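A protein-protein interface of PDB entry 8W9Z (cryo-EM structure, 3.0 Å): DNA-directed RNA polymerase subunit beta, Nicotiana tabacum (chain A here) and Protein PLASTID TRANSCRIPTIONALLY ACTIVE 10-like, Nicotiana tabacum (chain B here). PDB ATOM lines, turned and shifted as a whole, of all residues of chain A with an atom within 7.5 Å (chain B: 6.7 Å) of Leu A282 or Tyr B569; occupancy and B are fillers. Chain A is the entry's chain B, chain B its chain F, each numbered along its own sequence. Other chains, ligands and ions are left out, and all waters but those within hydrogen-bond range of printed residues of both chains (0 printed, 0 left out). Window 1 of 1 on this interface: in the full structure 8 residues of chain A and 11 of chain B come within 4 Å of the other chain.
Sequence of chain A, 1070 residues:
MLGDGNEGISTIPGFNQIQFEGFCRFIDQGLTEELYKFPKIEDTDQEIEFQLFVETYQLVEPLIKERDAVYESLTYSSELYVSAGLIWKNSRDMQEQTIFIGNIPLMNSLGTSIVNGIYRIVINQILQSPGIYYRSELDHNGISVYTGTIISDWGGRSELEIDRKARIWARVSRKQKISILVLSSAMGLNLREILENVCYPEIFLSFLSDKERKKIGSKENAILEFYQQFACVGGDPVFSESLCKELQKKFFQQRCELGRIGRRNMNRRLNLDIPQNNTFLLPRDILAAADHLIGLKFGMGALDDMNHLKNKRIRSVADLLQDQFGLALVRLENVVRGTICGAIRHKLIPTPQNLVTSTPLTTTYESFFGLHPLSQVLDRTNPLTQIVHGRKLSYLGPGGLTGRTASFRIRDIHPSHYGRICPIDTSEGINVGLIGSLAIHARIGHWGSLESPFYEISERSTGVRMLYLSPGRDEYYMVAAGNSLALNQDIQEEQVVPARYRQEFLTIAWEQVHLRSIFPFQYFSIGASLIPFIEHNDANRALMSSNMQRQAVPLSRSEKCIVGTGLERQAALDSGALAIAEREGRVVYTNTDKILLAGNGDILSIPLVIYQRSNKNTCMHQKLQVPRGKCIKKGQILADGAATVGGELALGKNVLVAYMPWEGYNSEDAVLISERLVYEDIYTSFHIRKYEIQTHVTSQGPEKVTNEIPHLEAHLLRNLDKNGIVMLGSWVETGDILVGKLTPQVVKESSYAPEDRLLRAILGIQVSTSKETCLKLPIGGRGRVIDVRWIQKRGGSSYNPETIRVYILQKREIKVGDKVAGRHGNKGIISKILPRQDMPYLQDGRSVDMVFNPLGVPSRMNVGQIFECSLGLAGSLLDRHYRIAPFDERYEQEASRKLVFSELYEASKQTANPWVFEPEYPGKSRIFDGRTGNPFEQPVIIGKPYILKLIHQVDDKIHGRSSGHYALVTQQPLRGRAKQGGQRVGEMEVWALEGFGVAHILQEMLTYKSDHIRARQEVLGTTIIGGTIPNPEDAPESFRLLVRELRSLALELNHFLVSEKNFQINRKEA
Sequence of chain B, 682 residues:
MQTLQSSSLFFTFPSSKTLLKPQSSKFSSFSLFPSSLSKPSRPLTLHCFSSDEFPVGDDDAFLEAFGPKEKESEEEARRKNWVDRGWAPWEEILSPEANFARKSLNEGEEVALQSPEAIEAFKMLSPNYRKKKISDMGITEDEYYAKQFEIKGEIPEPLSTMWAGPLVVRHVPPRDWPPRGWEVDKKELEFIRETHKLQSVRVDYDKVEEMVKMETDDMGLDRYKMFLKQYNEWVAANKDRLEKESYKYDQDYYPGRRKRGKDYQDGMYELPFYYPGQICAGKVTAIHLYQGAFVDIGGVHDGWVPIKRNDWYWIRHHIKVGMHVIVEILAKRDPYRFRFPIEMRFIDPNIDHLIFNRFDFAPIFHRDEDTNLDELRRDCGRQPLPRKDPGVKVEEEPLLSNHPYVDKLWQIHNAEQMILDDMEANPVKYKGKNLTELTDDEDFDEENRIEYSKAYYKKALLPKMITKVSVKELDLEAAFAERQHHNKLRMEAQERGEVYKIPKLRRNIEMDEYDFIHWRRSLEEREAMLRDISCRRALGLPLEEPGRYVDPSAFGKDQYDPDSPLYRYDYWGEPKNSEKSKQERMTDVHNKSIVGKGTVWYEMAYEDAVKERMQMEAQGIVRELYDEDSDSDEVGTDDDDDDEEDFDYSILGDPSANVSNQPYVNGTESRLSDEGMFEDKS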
ATOM      1  N   MET A 187      -2.415  31.489  40.126  1.00  0.00           N
ATOM      2  CA  MET A 187      -2.439  30.741  38.875  1.00  0.00           C
ATOM      3  C   MET A 187      -1.377  31.215  37.892  1.00  0.00           C
ATOM      4  O   MET A 187      -1.014  30.463  36.981  1.00  0.00           O
ATOM      5  CB  MET A 187      -3.823  30.839  38.229  1.00  0.00           C
ATOM      6  N   CYS A 256      -7.645  20.065  37.112  1.00  0.00           N
ATOM      7  CA  CYS A 256      -7.250  20.683  35.850  1.00  0.00           C
ATOM      8  C   CYS A 256      -7.345  19.704  34.688  1.00  0.00           C
ATOM      9  O   CYS A 256      -7.520  20.124  33.539  1.00  0.00           O
ATOM     10  CB  CYS A 256      -5.830  21.239  35.960  1.00  0.00           C
ATOM     11  N   LEU A 258      -9.215  18.091  32.690  1.00  0.00           N
ATOM     12  CA  LEU A 258     -10.547  17.954  32.121  1.00  0.00           C
ATOM     13  C   LEU A 258     -10.518  17.011  30.927  1.00  0.00           C
ATOM     14  O   LEU A 258      -9.521  16.915  30.206  1.00  0.00           O
ATOM     15  CB  LEU A 258     -11.098  19.315  31.695  1.00  0.00           C
ATOM     16  CG  LEU A 258     -11.358  20.340  32.799  1.00  0.00           C
ATOM     17  CD1 LEU A 258     -11.935  21.618  32.212  1.00  0.00           C
ATOM     18  CD2 LEU A 258     -12.287  19.766  33.855  1.00  0.00           C
ATOM     19  N   ARG A 263     -14.094  19.920  27.902  1.00  0.00           N
ATOM     20  CA  ARG A 263     -13.721  21.135  27.188  1.00  0.00           C
ATOM     21  C   ARG A 263     -14.843  21.597  26.268  1.00  0.00           C
ATOM     22  O   ARG A 263     -15.140  22.794  26.192  1.00  0.00           O
ATOM     23  CB  ARG A 263     -12.435  20.903  26.394  1.00  0.00           C
ATOM     24  CG  ARG A 263     -11.945  22.114  25.607  1.00  0.00           C
ATOM     25  CD  ARG A 263     -11.171  23.096  26.481  1.00  0.00           C
ATOM     26  NE  ARG A 263     -12.039  23.880  27.354  1.00  0.00           N
ATOM     27  CZ  ARG A 263     -11.602  24.790  28.219  1.00  0.00           C
ATOM     28  NH1 ARG A 263     -10.304  25.034  28.328  1.00  0.00           N
ATOM     29  NH2 ARG A 263     -12.464  25.458  28.973  1.00  0.00           N
ATOM     30  N   MET A 266     -17.629  23.079  28.396  1.00  0.00           N
ATOM     31  CA  MET A 266     -17.261  24.376  28.952  1.00  0.00           C
ATOM     32  C   MET A 266     -17.225  25.457  27.880  1.00  0.00           C
ATOM     33  O   MET A 266     -17.565  26.612  28.157  1.00  0.00           O
ATOM     34  CB  MET A 266     -15.914  24.279  29.666  1.00  0.00           C
ATOM     35  CG  MET A 266     -15.534  25.527  30.443  1.00  0.00           C
ATOM     36  SD  MET A 266     -14.119  25.268  31.527  1.00  0.00           S
ATOM     37  CE  MET A 266     -14.780  24.042  32.652  1.00  0.00           C
ATOM     38  N   LEU A 272     -16.061  30.854  25.446  1.00  0.00           N
ATOM     39  CA  LEU A 272     -14.664  30.716  25.064  1.00  0.00           C
ATOM     40  C   LEU A 272     -14.536  29.992  23.729  1.00  0.00           C
ATOM     41  O   LEU A 272     -15.426  29.246  23.312  1.00  0.00           O
ATOM     42  CB  LEU A 272     -13.876  29.963  26.137  1.00  0.00           C
ATOM     43  CG  LEU A 272     -13.530  30.723  27.419  1.00  0.00           C
ATOM     44  CD1 LEU A 272     -14.698  30.734  28.391  1.00  0.00           C
ATOM     45  CD2 LEU A 272     -12.289  30.138  28.071  1.00  0.00           C
ATOM     46  N   ILE A 274     -11.549  28.181  23.023  1.00  0.00           N
ATOM     47  CA  ILE A 274     -10.329  27.389  23.216  1.00  0.00           C
ATOM     48  C   ILE A 274     -10.372  26.174  22.296  1.00  0.00           C
ATOM     49  O   ILE A 274     -11.425  25.518  22.196  1.00  0.00           O
ATOM     50  CB  ILE A 274     -10.197  26.969  24.682  1.00  0.00           C
ATOM     51  CG1 ILE A 274     -10.141  28.203  25.584  1.00  0.00           C
ATOM     52  CG2 ILE A 274      -8.965  26.102  24.890  1.00  0.00           C
ATOM     53  CD1 ILE A 274      -8.981  29.127  25.285  1.00  0.00           C
ATOM     54  N   PRO A 275      -9.283  25.847  21.599  1.00  0.00           N
ATOM     55  CA  PRO A 275      -9.302  24.686  20.701  1.00  0.00           C
ATOM     56  C   PRO A 275      -9.587  23.392  21.450  1.00  0.00           C
ATOM     57  O   PRO A 275      -9.375  23.275  22.658  1.00  0.00           O
ATOM     58  CB  PRO A 275      -7.892  24.680  20.098  1.00  0.00           C
ATOM     59  CG  PRO A 275      -7.432  26.096  20.210  1.00  0.00           C
ATOM     60  CD  PRO A 275      -8.030  26.612  21.486  1.00  0.00           C
ATOM     61  N   ASN A 278      -6.739  21.351  23.550  1.00  0.00           N
ATOM     62  CA  ASN A 278      -6.459  21.694  24.937  1.00  0.00           C
ATOM     63  C   ASN A 278      -7.461  21.015  25.862  1.00  0.00           C
ATOM     64  O   ASN A 278      -8.675  21.145  25.682  1.00  0.00           O
ATOM     65  CB  ASN A 278      -6.505  23.210  25.128  1.00  0.00           C
ATOM     66  CG  ASN A 278      -5.523  23.939  24.233  1.00  0.00           C
ATOM     67  OD1 ASN A 278      -4.370  24.159  24.606  1.00  0.00           O
ATOM     68  ND2 ASN A 278      -5.976  24.320  23.045  1.00  0.00           N
ATOM     69  N   THR A 279      -6.949  20.283  26.852  1.00  0.00           N
ATOM     70  CA  THR A 279      -7.785  19.565  27.808  1.00  0.00           C
ATOM     71  C   THR A 279      -7.413  19.923  29.242  1.00  0.00           C
ATOM     72  O   THR A 279      -7.642  19.135  30.164  1.00  0.00           O
ATOM     73  CB  THR A 279      -7.689  18.054  27.596  1.00  0.00           C
ATOM     74  OG1 THR A 279      -6.320  17.641  27.701  1.00  0.00           O
ATOM     75  CG2 THR A 279      -8.227  17.668  26.226  1.00  0.00           C
ATOM     76  N   PHE A 280      -6.839  21.105  29.448  1.00  0.00           N
ATOM     77  CA  PHE A 280      -6.425  21.559  30.766  1.00  0.00           C
ATOM     78  C   PHE A 280      -7.237  22.779  31.179  1.00  0.00           C
ATOM     79  O   PHE A 280      -7.599  23.617  30.346  1.00  0.00           O
ATOM     80  CB  PHE A 280      -4.928  21.894  30.795  1.00  0.00           C
ATOM     81  CG  PHE A 280      -4.036  20.697  30.641  1.00  0.00           C
ATOM     82  CD1 PHE A 280      -4.489  19.430  30.970  1.00  0.00           C
ATOM     83  CD2 PHE A 280      -2.741  20.838  30.169  1.00  0.00           C
ATOM     84  CE1 PHE A 280      -3.669  18.326  30.831  1.00  0.00           C
ATOM     85  CE2 PHE A 280      -1.916  19.738  30.027  1.00  0.00           C
ATOM     86  CZ  PHE A 280      -2.381  18.480  30.357  1.00  0.00           C
ATOM     87  N   LEU A 281      -7.520  22.871  32.475  1.00  0.00           N
ATOM     88  CA  LEU A 281      -8.299  23.977  33.027  1.00  0.00           C
ATOM     89  C   LEU A 281      -7.435  25.230  33.050  1.00  0.00           C
ATOM     90  O   LEU A 281      -6.549  25.376  33.894  1.00  0.00           O
ATOM     91  CB  LEU A 281      -8.800  23.628  34.424  1.00  0.00           C
ATOM     92  CG  LEU A 281      -9.739  24.639  35.084  1.00  0.00           C
ATOM     93  CD1 LEU A 281     -11.042  24.740  34.308  1.00  0.00           C
ATOM     94  CD2 LEU A 281     -10.001  24.262  36.533  1.00  0.00           C
ATOM     95  N   LEU A 282      -7.692  26.141  32.121  1.00  0.00           N
ATOM     96  CA  LEU A 282      -6.938  27.378  32.034  1.00  0.00           C
ATOM     97  C   LEU A 282      -7.475  28.400  33.035  1.00  0.00           C
ATOM     98  O   LEU A 282      -8.639  28.331  33.437  1.00  0.00           O
ATOM     99  CB  LEU A 282      -7.021  27.947  30.622  1.00  0.00           C
ATOM    100  CG  LEU A 282      -6.808  26.943  29.487  1.00  0.00           C
ATOM    101  CD1 LEU A 282      -6.979  27.615  28.134  1.00  0.00           C
ATOM    102  CD2 LEU A 282      -5.443  26.282  29.596  1.00  0.00           C
ATOM    103  N   PRO A 283      -6.641  29.352  33.465  1.00  0.00           N
ATOM    104  CA  PRO A 283      -7.148  30.412  34.353  1.00  0.00           C
ATOM    105  C   PRO A 283      -8.244  31.246  33.717  1.00  0.00           C
ATOM    106  O   PRO A 283      -9.100  31.786  34.433  1.00  0.00           O
ATOM    107  CB  PRO A 283      -5.896  31.249  34.648  1.00  0.00           C
ATOM    108  CG  PRO A 283      -4.756  30.312  34.425  1.00  0.00           C
ATOM    109  CD  PRO A 283      -5.181  29.430  33.291  1.00  0.00           C
ATOM    110  N   ARG A 284      -8.241  31.371  32.387  1.00  0.00           N
ATOM    111  CA  ARG A 284      -9.323  32.072  31.708  1.00  0.00           C
ATOM    112  C   ARG A 284     -10.660  31.383  31.939  1.00  0.00           C
ATOM    113  O   ARG A 284     -11.702  32.044  31.960  1.00  0.00           O
ATOM    114  CB  ARG A 284      -9.019  32.177  30.212  1.00  0.00           C
ATOM    115  CG  ARG A 284      -9.983  33.054  29.432  1.00  0.00           C
ATOM    116  CD  ARG A 284      -9.418  33.400  28.062  1.00  0.00           C
ATOM    117  NE  ARG A 284     -10.308  34.275  27.305  1.00  0.00           N
ATOM    118  CZ  ARG A 284     -11.114  33.861  26.333  1.00  0.00           C
ATOM    119  NH1 ARG A 284     -11.141  32.581  25.990  1.00  0.00           N
ATOM    120  NH2 ARG A 284     -11.890  34.730  25.698  1.00  0.00           N
ATOM    121  N   ASP A 285     -10.650  30.062  32.134  1.00  0.00           N
ATOM    122  CA  ASP A 285     -11.884  29.349  32.448  1.00  0.00           C
ATOM    123  C   ASP A 285     -12.463  29.821  33.775  1.00  0.00           C
ATOM    124  O   ASP A 285     -13.661  30.106  33.876  1.00  0.00           O
ATOM    125  CB  ASP A 285     -11.628  27.842  32.480  1.00  0.00           C
ATOM    126  CG  ASP A 285     -11.022  27.324  31.192  1.00  0.00           C
ATOM    127  OD1 ASP A 285     -11.359  27.859  30.116  1.00  0.00           O
ATOM    128  OD2 ASP A 285     -10.207  26.380  31.255  1.00  0.00           O
ATOM    129  N   ILE A 286     -11.621  29.917  34.807  1.00  0.00           N
ATOM    130  CA  ILE A 286     -12.093  30.383  36.108  1.00  0.00           C
ATOM    131  C   ILE A 286     -12.505  31.848  36.033  1.00  0.00           C
ATOM    132  O   ILE A 286     -13.480  32.268  36.670  1.00  0.00           O
ATOM    133  CB  ILE A 286     -11.016  30.148  37.185  1.00  0.00           C
ATOM    134  CG1 ILE A 286     -10.759  28.651  37.379  1.00  0.00           C
ATOM    135  CG2 ILE A 286     -11.424  30.782  38.507  1.00  0.00           C
ATOM    136  CD1 ILE A 286      -9.604  28.108  36.562  1.00  0.00           C
ATOM    137  N   LEU A 287     -11.778  32.647  35.247  1.00  0.00           N
ATOM    138  CA  LEU A 287     -12.148  34.049  35.072  1.00  0.00           C
ATOM    139  C   LEU A 287     -13.539  34.173  34.459  1.00  0.00           C
ATOM    140  O   LEU A 287     -14.385  34.928  34.953  1.00  0.00           O
ATOM    141  CB  LEU A 287     -11.103  34.758  34.208  1.00  0.00           C
ATOM    142  CG  LEU A 287     -11.249  36.265  33.984  1.00  0.00           C
ATOM    143  CD1 LEU A 287      -9.884  36.933  33.998  1.00  0.00           C
ATOM    144  CD2 LEU A 287     -11.964  36.558  32.672  1.00  0.00           C
ATOM    145  N   ALA A 288     -13.795  33.430  33.380  1.00  0.00           N
ATOM    146  CA  ALA A 288     -15.105  33.470  32.742  1.00  0.00           C
ATOM    147  C   ALA A 288     -16.188  32.891  33.641  1.00  0.00           C
ATOM    148  O   ALA A 288     -17.334  33.350  33.598  1.00  0.00           O
ATOM    149  CB  ALA A 288     -15.066  32.724  31.410  1.00  0.00           C
ATOM    150  N   ASP B 561      -1.021  31.290  21.997  1.00  0.00           N
ATOM    151  CA  ASP B 561      -0.163  30.219  22.439  1.00  0.00           C
ATOM    152  C   ASP B 561       0.464  30.638  23.746  1.00  0.00           C
ATOM    153  O   ASP B 561       0.686  29.812  24.625  1.00  0.00           O
ATOM    154  CB  ASP B 561       0.925  29.954  21.404  1.00  0.00           C
ATOM    155  N   PRO B 562       0.779  31.931  23.872  1.00  0.00           N
ATOM    156  CA  PRO B 562       1.482  32.339  25.087  1.00  0.00           C
ATOM    157  C   PRO B 562       0.697  32.057  26.357  1.00  0.00           C
ATOM    158  O   PRO B 562      -0.506  32.307  26.408  1.00  0.00           O
ATOM    159  CB  PRO B 562       1.652  33.839  24.882  1.00  0.00           C
ATOM    160  N   ASP B 563       1.375  31.531  27.370  1.00  0.00           N
ATOM    161  CA  ASP B 563       0.725  31.187  28.631  1.00  0.00           C
ATOM    162  C   ASP B 563       0.168  32.381  29.371  1.00  0.00           C
ATOM    163  O   ASP B 563      -0.908  32.306  29.958  1.00  0.00           O
ATOM    164  CB  ASP B 563       1.718  30.457  29.529  1.00  0.00           C
ATOM    165  CG  ASP B 563       2.306  29.225  28.870  1.00  0.00           C
ATOM    166  OD1 ASP B 563       1.891  28.882  27.745  1.00  0.00           O
ATOM    167  OD2 ASP B 563       3.185  28.590  29.487  1.00  0.00           O
ATOM    168  N   SER B 564       0.891  33.487  29.343  1.00  0.00           N
ATOM    169  CA  SER B 564       0.482  34.670  30.096  1.00  0.00           C
ATOM    170  C   SER B 564      -0.863  35.242  29.696  1.00  0.00           C
ATOM    171  O   SER B 564      -1.587  35.735  30.549  1.00  0.00           O
ATOM    172  CB  SER B 564       1.570  35.744  30.063  1.00  0.00           C
ATOM    173  N   LEU B 566      -3.353  33.660  29.281  1.00  0.00           N
ATOM    174  CA  LEU B 566      -4.322  32.807  29.985  1.00  0.00           C
ATOM    175  C   LEU B 566      -5.035  31.978  28.963  1.00  0.00           C
ATOM    176  O   LEU B 566      -5.880  31.162  29.306  1.00  0.00           O
ATOM    177  CB  LEU B 566      -5.341  33.567  30.850  1.00  0.00           C
ATOM    178  CG  LEU B 566      -5.035  34.301  32.159  1.00  0.00           C
ATOM    179  CD1 LEU B 566      -4.495  35.700  31.915  1.00  0.00           C
ATOM    180  CD2 LEU B 566      -6.323  34.424  32.952  1.00  0.00           C
ATOM    181  N   TYR B 567      -4.676  32.155  27.699  1.00  0.00           N
ATOM    182  CA  TYR B 567      -5.256  31.335  26.662  1.00  0.00           C
ATOM    183  C   TYR B 567      -4.462  30.068  26.686  1.00  0.00           C
ATOM    184  O   TYR B 567      -4.778  29.120  25.978  1.00  0.00           O
ATOM    185  CB  TYR B 567      -5.166  32.009  25.316  1.00  0.00           C
ATOM    186  CG  TYR B 567      -6.188  33.089  25.123  1.00  0.00           C
ATOM    187  CD1 TYR B 567      -5.933  34.386  25.529  1.00  0.00           C
ATOM    188  CD2 TYR B 567      -7.412  32.812  24.542  1.00  0.00           C
ATOM    189  CE1 TYR B 567      -6.868  35.383  25.359  1.00  0.00           C
ATOM    190  CE2 TYR B 567      -8.351  33.803  24.357  1.00  0.00           C
ATOM    191  CZ  TYR B 567      -8.074  35.087  24.773  1.00  0.00           C
ATOM    192  OH  TYR B 567      -9.005  36.082  24.607  1.00  0.00           O
ATOM    193  N   ARG B 568      -3.403  30.051  27.480  1.00  0.00           N
ATOM    194  CA  ARG B 568      -2.633  28.834  27.642  1.00  0.00           C
ATOM    195  C   ARG B 568      -2.364  28.620  29.117  1.00  0.00           C
ATOM    196  O   ARG B 568      -2.408  29.563  29.905  1.00  0.00           O
ATOM    197  CB  ARG B 568      -1.340  28.880  26.848  1.00  0.00           C
ATOM    198  N   TYR B 569      -2.046  27.387  29.489  1.00  0.00           N
ATOM    199  CA  TYR B 569      -1.869  27.067  30.901  1.00  0.00           C
ATOM    200  C   TYR B 569      -0.604  27.562  31.534  1.00  0.00           C
ATOM    201  O   TYR B 569       0.428  27.672  30.887  1.00  0.00           O
ATOM    202  CB  TYR B 569      -2.008  25.558  31.147  1.00  0.00           C
ATOM    203  CG  TYR B 569      -1.335  24.674  30.122  1.00  0.00           C
ATOM    204  CD1 TYR B 569      -2.010  24.265  28.979  1.00  0.00           C
ATOM    205  CD2 TYR B 569      -0.034  24.231  30.306  1.00  0.00           C
ATOM    206  CE1 TYR B 569      -1.403  23.456  28.041  1.00  0.00           C
ATOM    207  CE2 TYR B 569       0.580  23.418  29.372  1.00  0.00           C
ATOM    208  CZ  TYR B 569      -0.109  23.034  28.244  1.00  0.00           C
ATOM    209  OH  TYR B 569       0.497  22.224  27.311  1.00  0.00           O
ATOM    210  N   ASP B 570      -0.684  27.837  32.822  1.00  0.00           N
ATOM    211  CA  ASP B 570       0.477  28.285  33.546  1.00  0.00           C
ATOM    212  C   ASP B 570       0.473  27.403  34.758  1.00  0.00           C
ATOM    213  O   ASP B 570      -0.564  26.837  35.104  1.00  0.00           O
ATOM    214  CB  ASP B 570       0.322  29.743  33.949  1.00  0.00           C
ATOM    215  N   TYR B 571       1.615  27.257  35.409  1.00  0.00           N
ATOM    216  CA  TYR B 571       1.671  26.330  36.518  1.00  0.00           C
ATOM    217  C   TYR B 571       0.722  26.705  37.630  1.00  0.00           C
ATOM    218  O   TYR B 571       0.708  27.845  38.082  1.00  0.00           O
ATOM    219  CB  TYR B 571       3.091  26.260  37.065  1.00  0.00           C
ATOM    220  N   PRO B 575       1.927  23.329  38.345  1.00  0.00           N
ATOM    221  CA  PRO B 575       1.598  22.484  37.192  1.00  0.00           C
ATOM    222  C   PRO B 575       2.307  22.909  35.921  1.00  0.00           C
ATOM    223  O   PRO B 575       1.687  23.522  35.056  1.00  0.00           O
ATOM    224  CB  PRO B 575       0.107  22.714  37.004  1.00  0.00           C
ATOM    225  N   LYS B 576       3.576  22.560  35.785  1.00  0.00           N
ATOM    226  CA  LYS B 576       4.312  22.888  34.576  1.00  0.00           C
ATOM    227  C   LYS B 576       4.171  21.784  33.545  1.00  0.00           C
ATOM    228  O   LYS B 576       4.706  21.892  32.444  1.00  0.00           O
ATOM    229  CB  LYS B 576       5.784  23.108  34.899  1.00  0.00           C
ATOM    230  N   ASN B 577       3.453  20.721  33.889  1.00  0.00           N
ATOM    231  CA  ASN B 577       3.317  19.585  32.983  1.00  0.00           C
ATOM    232  C   ASN B 577       2.633  19.981  31.694  1.00  0.00           C
ATOM    233  O   ASN B 577       1.690  20.769  31.696  1.00  0.00           O
ATOM    234  CB  ASN B 577       2.522  18.461  33.646  1.00  0.00           C
ATOM    235  N   SER B 578       3.108  19.427  30.587  1.00  0.00           N
ATOM    236  CA  SER B 578       2.534  19.767  29.297  1.00  0.00           C
ATOM    237  C   SER B 578       1.944  18.560  28.593  1.00  0.00           C
ATOM    238  O   SER B 578       2.601  17.528  28.467  1.00  0.00           O
ATOM    239  CB  SER B 578       3.593  20.427  28.411  1.00  0.00           C
ATOM    240  N   GLU B 579       0.710  18.697  28.115  1.00  0.00           N
ATOM    241  CA  GLU B 579       0.051  17.604  27.405  1.00  0.00           C
ATOM    242  C   GLU B 579       0.691  17.361  26.071  1.00  0.00           C
ATOM    243  O   GLU B 579       1.050  18.314  25.376  1.00  0.00           O
ATOM    244  CB  GLU B 579      -1.421  17.924  27.161  1.00  0.00           C
ATOM    245  N   LYS B 580       0.852  16.092  25.718  1.00  0.00           N
ATOM    246  CA  LYS B 580       1.407  15.752  24.423  1.00  0.00           C
ATOM    247  C   LYS B 580       2.712  16.488  24.275  1.00  0.00           C
ATOM    248  O   LYS B 580       3.550  16.440  25.183  1.00  0.00           O
ATOM    249  CB  LYS B 580       0.448  16.092  23.279  1.00  0.00           C
ATOM    250  N   SER B 581       2.901  17.142  23.128  1.00  0.00           N
ATOM    251  CA  SER B 581       4.126  17.888  22.883  1.00  0.00           C
ATOM    252  C   SER B 581       5.212  16.896  23.173  1.00  0.00           C
ATOM    253  O   SER B 581       6.211  17.227  23.809  1.00  0.00           O
ATOM    254  CB  SER B 581       4.230  19.120  23.779  1.00  0.00           C
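OH of Tyr B567 sits at hydrogen-bond distance from NH2 of Arg A284 (3.4 Å). The backbone carbonyl oxygen (O) of Met A187 sits close to the backbone carbonyl oxygen (O) of Tyr B571, at 3.3 Å.
The backbone NH (N) of Leu A282 lies within hydrogen-bond range of the side-chain carboxylate (OD2) of Asp A285 (2.7 Å).
Asp B570 touches Met A187 (CB to O, 3.4 Å). Tyr B569 touches Phe A280. CZ of Phe A280 touches CB of Glu B579, at 3.4 Å. Leu B566 touches Leu A282 (O to CB, 3.7 Å). Leu A282 touches Tyr B567. C of Arg B568 touches CD2 of Leu A282, 3.9 Å away. Tyr B569 touches Leu A282. CD2 of Leu B566 touches CB of Pro A283 (3.6 Å). Leu B566 touches Arg A284 (O to CB, 3.4 Å).
Of the printed residues of chain B, Met A187 touches Asp B570 and Tyr B571. Printed residues of chain B within 4 Å of Leu A282: Leu B566 (3.7 Å), Tyr B567 (3.4 Å), Arg B568 (3.9 Å) and Tyr B569 (3.6 Å). Of the printed residues of chain B, Arg A284 touches Leu B566 and Tyr B567. Of the printed residues of chain A, Leu B566 touches Leu A282, Pro A283 and Arg A284. Of the printed residues of chain A, Tyr B567 touches Leu A282 (3.4 Å) and Arg A284 (3.4 Å). Tyr B569 touches just these residues of chain A: Phe A280 and Leu A282. Of the printed residues of chain A, Tyr B571 touches Met A187. Ser B578 touches none of the printed residues of chain A. The nearest printed residue of chain A that does not touch Glu B579 is Thr A279 (4.9 Å).
Printed residues of chain A that touch a printed residue of chain B: Met A187, Phe A280, Leu A282, Pro A283 and Arg A284. Hydrophobic or aromatic side chains of chain A within 4 Å of the printed part of chain B: Phe A280, Leu A282 and Pro A283. Hydrophobic or aromatic side chains of chain B that line the printed part of chain A: Leu B566, Tyr B567 and Tyr B569. Among the printed residues, 11 pairs touch across the chains. Among the printed residues, no Asp or Glu carboxylate lies within 4 Å of a Lys or Arg side-chain nitrogen of the other chain.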
